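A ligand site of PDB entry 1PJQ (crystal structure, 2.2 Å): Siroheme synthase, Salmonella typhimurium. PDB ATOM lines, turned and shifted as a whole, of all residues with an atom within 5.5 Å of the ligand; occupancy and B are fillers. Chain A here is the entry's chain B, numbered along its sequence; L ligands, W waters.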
ATOM      1  N   PRO A 225     -20.788 -12.658  -0.046  1.00  0.00           N
ATOM      2  CA  PRO A 225     -19.862 -12.467  -1.160  1.00  0.00           C
ATOM      3  C   PRO A 225     -20.247 -11.482  -2.276  1.00  0.00           C
ATOM      4  O   PRO A 225     -19.412 -11.145  -3.115  1.00  0.00           O
ATOM      5  CB  PRO A 225     -19.659 -13.888  -1.681  1.00  0.00           C
ATOM      6  CG  PRO A 225     -20.980 -14.534  -1.393  1.00  0.00           C
ATOM      7  CD  PRO A 225     -21.302 -14.040  -0.017  1.00  0.00           C
ATOM      8  N   GLY A 226     -21.489 -11.024  -2.308  1.00  0.00           N
ATOM      9  CA  GLY A 226     -21.886 -10.074  -3.352  1.00  0.00           C
ATOM     10  C   GLY A 226     -23.366 -10.053  -3.675  1.00  0.00           C
ATOM     11  O   GLY A 226     -23.988  -8.989  -3.725  1.00  0.00           O
ATOM     12  N   LEU A 250     -15.304  -4.805  -0.867  1.00  0.00           N
ATOM     13  CA  LEU A 250     -15.879  -6.119  -1.141  1.00  0.00           C
ATOM     14  C   LEU A 250     -17.351  -6.249  -0.745  1.00  0.00           C
ATOM     15  O   LEU A 250     -17.908  -7.350  -0.714  1.00  0.00           O
ATOM     16  CB  LEU A 250     -15.049  -7.228  -0.493  1.00  0.00           C
ATOM     17  CG  LEU A 250     -13.715  -7.464  -1.201  1.00  0.00           C
ATOM     18  CD1 LEU A 250     -13.105  -8.755  -0.719  1.00  0.00           C
ATOM     19  CD2 LEU A 250     -13.932  -7.522  -2.712  1.00  0.00           C
ATOM     20  N   GLY A 301     -17.359  -7.490   3.874  1.00  0.00           N
ATOM     21  CA  GLY A 301     -17.528  -8.448   2.789  1.00  0.00           C
ATOM     22  C   GLY A 301     -17.547  -9.864   3.353  1.00  0.00           C
ATOM     23  O   GLY A 301     -16.785 -10.166   4.267  1.00  0.00           O
ATOM     24  N   GLY A 302     -18.410 -10.736   2.822  1.00  0.00           N
ATOM     25  CA  GLY A 302     -18.488 -12.107   3.317  1.00  0.00           C
ATOM     26  C   GLY A 302     -18.816 -12.219   4.811  1.00  0.00           C
ATOM     27  O   GLY A 302     -19.840 -11.714   5.248  1.00  0.00           O
ATOM     28  N   ASP A 303     -17.950 -12.885   5.580  1.00  0.00           N
ATOM     29  CA  ASP A 303     -18.180 -13.027   7.029  1.00  0.00           C
ATOM     30  C   ASP A 303     -17.184 -12.174   7.832  1.00  0.00           C
ATOM     31  O   ASP A 303     -16.027 -12.034   7.446  1.00  0.00           O
ATOM     32  CB  ASP A 303     -18.079 -14.500   7.449  1.00  0.00           C
ATOM     33  CG  ASP A 303     -18.297 -14.688   8.939  1.00  0.00           C
ATOM     34  OD1 ASP A 303     -17.302 -14.760   9.703  1.00  0.00           O
ATOM     35  OD2 ASP A 303     -19.479 -14.745   9.366  1.00  0.00           O
ATOM     36  N   PRO A 304     -17.636 -11.579   8.949  1.00  0.00           N
ATOM     37  CA  PRO A 304     -16.838 -10.718   9.841  1.00  0.00           C
ATOM     38  C   PRO A 304     -15.639 -11.346  10.559  1.00  0.00           C
ATOM     39  O   PRO A 304     -14.634 -10.669  10.781  1.00  0.00           O
ATOM     40  CB  PRO A 304     -17.876 -10.204  10.847  1.00  0.00           C
ATOM     41  CG  PRO A 304     -19.181 -10.314  10.121  1.00  0.00           C
ATOM     42  CD  PRO A 304     -19.049 -11.622   9.395  1.00  0.00           C
ATOM     43  N   ILE A 306     -13.875 -14.212   9.514  1.00  0.00           N
ATOM     44  CA  ILE A 306     -13.081 -15.093   8.654  1.00  0.00           C
ATOM     45  C   ILE A 306     -12.183 -14.309   7.703  1.00  0.00           C
ATOM     46  O   ILE A 306     -12.575 -13.954   6.582  1.00  0.00           O
ATOM     47  CB  ILE A 306     -14.013 -16.048   7.835  1.00  0.00           C
ATOM     48  CG1 ILE A 306     -14.692 -17.022   8.805  1.00  0.00           C
ATOM     49  CG2 ILE A 306     -13.212 -16.836   6.801  1.00  0.00           C
ATOM     50  CD1 ILE A 306     -15.727 -17.925   8.173  1.00  0.00           C
ATOM     51  N   PHE A 307     -10.956 -14.066   8.148  1.00  0.00           N
ATOM     52  CA  PHE A 307      -9.985 -13.304   7.374  1.00  0.00           C
ATOM     53  C   PHE A 307     -10.585 -11.904   7.193  1.00  0.00           C
ATOM     54  O   PHE A 307     -10.323 -11.212   6.194  1.00  0.00           O
ATOM     55  CB  PHE A 307      -9.738 -13.958   6.003  1.00  0.00           C
ATOM     56  CG  PHE A 307      -9.219 -15.380   6.070  1.00  0.00           C
ATOM     57  CD1 PHE A 307      -9.849 -16.392   5.366  1.00  0.00           C
ATOM     58  CD2 PHE A 307      -8.089 -15.697   6.833  1.00  0.00           C
ATOM     59  CE1 PHE A 307      -9.368 -17.710   5.407  1.00  0.00           C
ATOM     60  CE2 PHE A 307      -7.598 -17.010   6.882  1.00  0.00           C
ATOM     61  CZ  PHE A 307      -8.241 -18.015   6.166  1.00  0.00           C
ATOM     62  N   GLY A 308     -11.385 -11.477   8.163  1.00  0.00           N
ATOM     63  CA  GLY A 308     -12.032 -10.187   8.095  1.00  0.00           C
ATOM     64  C   GLY A 308     -11.579  -9.151   9.110  1.00  0.00           C
ATOM     65  O   GLY A 308     -12.019  -7.996   9.074  1.00  0.00           O
ATOM     66  N   ILE A 330     -22.488 -15.095   4.818  1.00  0.00           N
ATOM     67  CA  ILE A 330     -22.022 -16.187   3.967  1.00  0.00           C
ATOM     68  C   ILE A 330     -20.582 -15.865   3.573  1.00  0.00           C
ATOM     69  O   ILE A 330     -20.316 -14.809   2.980  1.00  0.00           O
ATOM     70  CB  ILE A 330     -22.876 -16.282   2.676  1.00  0.00           C
ATOM     71  CG1 ILE A 330     -24.368 -16.471   3.030  1.00  0.00           C
ATOM     72  CG2 ILE A 330     -22.358 -17.415   1.794  1.00  0.00           C
ATOM     73  CD1 ILE A 330     -24.719 -17.792   3.720  1.00  0.00           C
ATOM     74  N   THR A 331     -19.646 -16.759   3.901  1.00  0.00           N
ATOM     75  CA  THR A 331     -18.243 -16.530   3.587  1.00  0.00           C
ATOM     76  C   THR A 331     -18.017 -16.875   2.115  1.00  0.00           C
ATOM     77  O   THR A 331     -18.764 -17.662   1.524  1.00  0.00           O
ATOM     78  CB  THR A 331     -17.331 -17.406   4.501  1.00  0.00           C
ATOM     79  OG1 THR A 331     -15.962 -16.970   4.403  1.00  0.00           O
ATOM     80  CG2 THR A 331     -17.438 -18.873   4.080  1.00  0.00           C
ATOM     81  N   ALA A 332     -16.988 -16.289   1.509  1.00  0.00           N
ATOM     82  CA  ALA A 332     -16.674 -16.525   0.100  1.00  0.00           C
ATOM     83  C   ALA A 332     -16.569 -18.021  -0.249  1.00  0.00           C
ATOM     84  O   ALA A 332     -16.986 -18.444  -1.315  1.00  0.00           O
ATOM     85  CB  ALA A 332     -15.383 -15.814  -0.245  1.00  0.00           C
ATOM     86  N   ALA A 333     -16.009 -18.809   0.666  1.00  0.00           N
ATOM     87  CA  ALA A 333     -15.871 -20.247   0.439  1.00  0.00           C
ATOM     88  C   ALA A 333     -17.242 -20.880   0.193  1.00  0.00           C
ATOM     89  O   ALA A 333     -17.431 -21.637  -0.757  1.00  0.00           O
ATOM     90  CB  ALA A 333     -15.169 -20.900   1.640  1.00  0.00           C
ATOM     91  N   CYS A 336     -18.991 -19.270  -3.270  1.00  0.00           N
ATOM     92  CA  CYS A 336     -18.377 -19.795  -4.487  1.00  0.00           C
ATOM     93  C   CYS A 336     -18.621 -21.290  -4.653  1.00  0.00           C
ATOM     94  O   CYS A 336     -18.792 -21.769  -5.762  1.00  0.00           O
ATOM     95  CB  CYS A 336     -16.857 -19.550  -4.479  1.00  0.00           C
ATOM     96  SG  CYS A 336     -16.380 -17.814  -4.504  1.00  0.00           S
ATOM     97  N   PHE A 380      -8.091 -21.310  -0.928  1.00  0.00           N
ATOM     98  CA  PHE A 380      -7.235 -20.172  -0.647  1.00  0.00           C
ATOM     99  C   PHE A 380      -7.876 -18.808  -0.850  1.00  0.00           C
ATOM    100  O   PHE A 380      -8.423 -18.514  -1.919  1.00  0.00           O
ATOM    101  CB  PHE A 380      -5.968 -20.219  -1.521  1.00  0.00           C
ATOM    102  CG  PHE A 380      -5.190 -21.498  -1.399  1.00  0.00           C
ATOM    103  CD1 PHE A 380      -5.629 -22.662  -2.031  1.00  0.00           C
ATOM    104  CD2 PHE A 380      -4.021 -21.555  -0.654  1.00  0.00           C
ATOM    105  CE1 PHE A 380      -4.921 -23.855  -1.910  1.00  0.00           C
ATOM    106  CE2 PHE A 380      -3.299 -22.752  -0.535  1.00  0.00           C
ATOM    107  CZ  PHE A 380      -3.756 -23.898  -1.170  1.00  0.00           C
ATOM    108  N   TYR A 381      -7.812 -17.967   0.186  1.00  0.00           N
ATOM    109  CA  TYR A 381      -8.322 -16.596   0.143  1.00  0.00           C
ATOM    110  C   TYR A 381      -7.086 -15.721  -0.097  1.00  0.00           C
ATOM    111  O   TYR A 381      -6.038 -15.953   0.505  1.00  0.00           O
ATOM    112  CB  TYR A 381      -8.918 -16.172   1.490  1.00  0.00           C
ATOM    113  CG  TYR A 381     -10.298 -16.681   1.825  1.00  0.00           C
ATOM    114  CD1 TYR A 381     -10.518 -18.035   2.121  1.00  0.00           C
ATOM    115  CD2 TYR A 381     -11.380 -15.806   1.907  1.00  0.00           C
ATOM    116  CE1 TYR A 381     -11.792 -18.488   2.484  1.00  0.00           C
ATOM    117  CE2 TYR A 381     -12.644 -16.253   2.278  1.00  0.00           C
ATOM    118  CZ  TYR A 381     -12.845 -17.589   2.564  1.00  0.00           C
ATOM    119  OH  TYR A 381     -14.105 -18.027   2.937  1.00  0.00           O
ATOM    120  N   MET A 382      -7.206 -14.725  -0.971  1.00  0.00           N
ATOM    121  CA  MET A 382      -6.107 -13.822  -1.284  1.00  0.00           C
ATOM    122  C   MET A 382      -4.859 -14.562  -1.749  1.00  0.00           C
ATOM    123  O   MET A 382      -3.763 -14.298  -1.262  1.00  0.00           O
ATOM    124  CB  MET A 382      -5.730 -12.999  -0.043  1.00  0.00           C
ATOM    125  CG  MET A 382      -6.867 -12.229   0.602  1.00  0.00           C
ATOM    126  SD  MET A 382      -6.474 -11.743   2.294  1.00  0.00           S
ATOM    127  CE  MET A 382      -6.651 -13.316   3.141  1.00  0.00           C
ATOM    128  N   GLY A 383      -5.007 -15.484  -2.695  1.00  0.00           N
ATOM    129  CA  GLY A 383      -3.858 -16.233  -3.168  1.00  0.00           C
ATOM    130  C   GLY A 383      -3.606 -16.183  -4.662  1.00  0.00           C
ATOM    131  O   GLY A 383      -2.870 -17.018  -5.184  1.00  0.00           O
ATOM    132  N   VAL A 408     -12.565 -19.210  -8.827  1.00  0.00           N
ATOM    133  CA  VAL A 408     -13.853 -18.543  -8.911  1.00  0.00           C
ATOM    134  C   VAL A 408     -13.690 -17.050  -8.629  1.00  0.00           C
ATOM    135  O   VAL A 408     -13.325 -16.665  -7.514  1.00  0.00           O
ATOM    136  CB  VAL A 408     -14.857 -19.150  -7.888  1.00  0.00           C
ATOM    137  CG1 VAL A 408     -16.274 -18.563  -8.099  1.00  0.00           C
ATOM    138  CG2 VAL A 408     -14.862 -20.672  -8.025  1.00  0.00           C
ATOM    139  N   GLU A 409     -13.951 -16.225  -9.638  1.00  0.00           N
ATOM    140  CA  GLU A 409     -13.839 -14.760  -9.537  1.00  0.00           C
ATOM    141  C   GLU A 409     -15.208 -14.125  -9.380  1.00  0.00           C
ATOM    142  O   GLU A 409     -16.134 -14.482 -10.101  1.00  0.00           O
ATOM    143  CB  GLU A 409     -13.173 -14.188 -10.785  1.00  0.00           C
ATOM    144  CG  GLU A 409     -13.391 -12.685 -11.000  1.00  0.00           C
ATOM    145  CD  GLU A 409     -12.720 -12.142 -12.269  1.00  0.00           C
ATOM    146  OE1 GLU A 409     -12.558 -12.908 -13.237  1.00  0.00           O
ATOM    147  OE2 GLU A 409     -12.380 -10.949 -12.314  1.00  0.00           O
ATOM    148  N   ASN A 410     -15.331 -13.164  -8.468  1.00  0.00           N
ATOM    149  CA  ASN A 410     -16.603 -12.476  -8.212  1.00  0.00           C
ATOM    150  C   ASN A 410     -17.743 -13.480  -7.959  1.00  0.00           C
ATOM    151  O   ASN A 410     -18.840 -13.351  -8.520  1.00  0.00           O
ATOM    152  CB  ASN A 410     -16.967 -11.555  -9.401  1.00  0.00           C
ATOM    153  CG  ASN A 410     -16.135 -10.267  -9.447  1.00  0.00           C
ATOM    154  OD1 ASN A 410     -15.853  -9.665  -8.418  1.00  0.00           O
ATOM    155  ND2 ASN A 410     -15.756  -9.853 -10.651  1.00  0.00           N
ATOM    156  N   GLY A 411     -17.470 -14.472  -7.120  1.00  0.00           N
ATOM    157  CA  GLY A 411     -18.463 -15.493  -6.814  1.00  0.00           C
ATOM    158  C   GLY A 411     -19.832 -14.951  -6.396  1.00  0.00           C
ATOM    159  O   GLY A 411     -19.914 -13.919  -5.707  1.00  0.00           O
ATOM    160  N   THR A 412     -20.870 -15.672  -6.796  1.00  0.00           N
ATOM    161  CA  THR A 412     -22.291 -15.368  -6.536  1.00  0.00           C
ATOM    162  C   THR A 412     -22.854 -14.119  -7.218  1.00  0.00           C
ATOM    163  O   THR A 412     -24.040 -13.837  -7.080  1.00  0.00           O
ATOM    164  CB  THR A 412     -22.630 -15.270  -5.007  1.00  0.00           C
ATOM    165  OG1 THR A 412     -22.238 -13.986  -4.507  1.00  0.00           O
ATOM    166  CG2 THR A 412     -21.940 -16.394  -4.201  1.00  0.00           C
ATOM    167  N   PRO A 436     -11.644  -9.988  -6.862  1.00  0.00           N
ATOM    168  CA  PRO A 436     -11.347 -11.017  -5.851  1.00  0.00           C
ATOM    169  C   PRO A 436     -11.656 -12.414  -6.393  1.00  0.00           C
ATOM    170  O   PRO A 436     -12.641 -12.594  -7.107  1.00  0.00           O
ATOM    171  CB  PRO A 436     -12.282 -10.669  -4.688  1.00  0.00           C
ATOM    172  CG  PRO A 436     -13.163  -9.510  -5.208  1.00  0.00           C
ATOM    173  CD  PRO A 436     -13.022  -9.514  -6.693  1.00  0.00           C
ATOM    174  N   ALA A 437     -10.836 -13.391  -6.018  1.00  0.00           N
ATOM    175  CA  ALA A 437     -11.027 -14.764  -6.453  1.00  0.00           C
ATOM    176  C   ALA A 437     -10.568 -15.759  -5.390  1.00  0.00           C
ATOM    177  O   ALA A 437      -9.785 -15.426  -4.515  1.00  0.00           O
ATOM    178  CB  ALA A 437     -10.270 -15.002  -7.755  1.00  0.00           C
ATOM    179  N   LEU A 438     -11.075 -16.989  -5.470  1.00  0.00           N
ATOM    180  CA  LEU A 438     -10.686 -18.039  -4.537  1.00  0.00           C
ATOM    181  C   LEU A 438     -10.084 -19.188  -5.329  1.00  0.00           C
ATOM    182  O   LEU A 438     -10.410 -19.400  -6.497  1.00  0.00           O
ATOM    183  CB  LEU A 438     -11.877 -18.595  -3.756  1.00  0.00           C
ATOM    184  CG  LEU A 438     -12.550 -17.854  -2.603  1.00  0.00           C
ATOM    185  CD1 LEU A 438     -13.663 -18.757  -2.086  1.00  0.00           C
ATOM    186  CD2 LEU A 438     -11.579 -17.521  -1.474  1.00  0.00           C
HETATM  187  N1  LIG L   1     -14.357 -11.953   5.227  1.00  0.00           N
HETATM  188  C1  LIG L   1     -14.398 -12.450   3.844  1.00  0.00           C
HETATM  189  C2  LIG L   1     -12.971 -12.696   3.329  1.00  0.00           C
HETATM  190  C3  LIG L   1     -12.154 -11.386   3.296  1.00  0.00           C
HETATM  191  S1  LIG L   1     -10.406 -11.641   2.763  1.00  0.00           S
HETATM  192  C4  LIG L   1     -15.201 -13.767   3.796  1.00  0.00           C
HETATM  193  O1  LIG L   1     -15.576 -14.263   4.886  1.00  0.00           O
HETATM  194  O2  LIG L   1     -15.425 -14.246   2.665  1.00  0.00           O
HETATM  195  C5  LIG L   1     -10.498 -11.204   0.992  1.00  0.00           C
HETATM  196  C6  LIG L   1     -10.599 -12.427   0.076  1.00  0.00           C
HETATM  197  O3  LIG L   1     -11.900 -13.097   0.126  1.00  0.00           O
HETATM  198  C7  LIG L   1     -10.417 -12.094  -1.386  1.00  0.00           C
HETATM  199  O4  LIG L   1      -9.013 -11.967  -1.681  1.00  0.00           O
HETATM  200  C8  LIG L   1     -10.981 -13.310  -2.088  1.00  0.00           C
HETATM  201  O5  LIG L   1     -10.011 -14.356  -2.115  1.00  0.00           O
HETATM  202  C9  LIG L   1     -12.155 -13.738  -1.189  1.00  0.00           C
HETATM  203  N2  LIG L   1     -13.449 -13.222  -1.759  1.00  0.00           N
HETATM  204  C10 LIG L   1     -14.241 -12.279  -1.211  1.00  0.00           C
HETATM  205  N3  LIG L   1     -15.330 -12.126  -1.970  1.00  0.00           N
HETATM  206  C11 LIG L   1     -15.235 -12.951  -3.010  1.00  0.00           C
HETATM  207  C12 LIG L   1     -16.069 -13.229  -4.097  1.00  0.00           C
HETATM  208  N4  LIG L   1     -17.229 -12.588  -4.238  1.00  0.00           N
HETATM  209  N5  LIG L   1     -15.697 -14.147  -5.015  1.00  0.00           N
HETATM  210  C13 LIG L   1     -14.424 -14.861  -4.849  1.00  0.00           C
HETATM  211  N6  LIG L   1     -13.650 -14.579  -3.789  1.00  0.00           N
HETATM  212  C14 LIG L   1     -14.039 -13.667  -2.872  1.00  0.00           C
HETATM  213  O   HOH W   1     -14.479  -9.138   5.105  1.00  0.00           O
HETATM  214  O   HOH W   2     -17.014 -10.243  -0.642  1.00  0.00           O
HETATM  215  O   HOH W   3      -8.573 -11.807  -4.567  1.00  0.00           O
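The side-chain hydroxyl (OG1) of Thr 331 sits at hydrogen-bond distance from the side-chain hydroxyl (OH) of Tyr 381 (2.6 Å). The side-chain carboxylate (OD1) of Asp 303 lies within hydrogen-bond range of the backbone NH (N) of Ile 306 (3.5 Å). The backbone carbonyl oxygen of Ala 332 sits at hydrogen-bond distance from the side-chain sulfur of Cys 336. The backbone NH of Ala 333 lies within hydrogen-bond range of the side-chain hydroxyl of Tyr 381. The backbone carbonyl oxygen (O) of Val 408 is in hydrogen-bond range of the backbone NH (N) of Leu 438, 3.1 Å away. The backbone NH of Asn 410 lies within hydrogen-bond range of the backbone carbonyl oxygen of Pro 436, 3.1 Å away.
Water W1 bridges O of Gly 301 (2.7 Å) and N1 of the ligand (2.8 Å). Water W2 bridges a nitrogen (N3) of the ligand (2.9 Å) and the backbone carbonyl oxygen of Leu 250 (3.0 Å). Water W3 lies within hydrogen-bond range of O4 of the ligand (2.9 Å) and N of Ala 437 (3.1 Å).
O of Ala 437 sits at hydrogen-bond distance from O5 of the ligand. A nitrogen (N5) of the ligand sits at hydrogen-bond distance from the backbone NH (N) of Gly 411 (2.8 Å). A nitrogen (N4) of the ligand sits at hydrogen-bond distance from the backbone carbonyl oxygen (O) of Gly 411. The side-chain hydroxyl of Thr 331 sits at hydrogen-bond distance from an oxygen (O1) of the ligand, 2.8 Å away. N of Asp 303 is in hydrogen-bond range of O1 of the ligand, at 2.8 Å. The backbone carbonyl oxygen (O) of Asp 303 sits at hydrogen-bond distance from a nitrogen (N1) of the ligand (2.8 Å). An oxygen (O2) of the ligand sits at hydrogen-bond distance from the backbone NH (N) of Ala 332. N4 of the ligand lies within hydrogen-bond range of O of Pro 225 (2.8 Å). N1 of the ligand sits at hydrogen-bond distance from O of Ile 306 (3.0 Å). An oxygen (O5) of the ligand is in hydrogen-bond range of the backbone NH (N) of Met 382 (3.1 Å). The backbone carbonyl oxygen (O) of Gly 301 lies within hydrogen-bond range of a nitrogen (N1) of the ligand, 3.2 Å away. A nitrogen (N5) of the ligand lies close to the side-chain sulfur (SG) of Cys 336 (3.8 Å).
The backbone carbonyl oxygen (O) of Phe 307 lies close to a sulfur (S1) of the ligand (3.5 Å). Merely in contact with the ligand: Leu 250, Gly 302, Tyr 381, Val 408, Asn 410, Pro 436 and Leu 438. Along chain A the residues within 4 Å of the ligand span positions 225 to 438.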
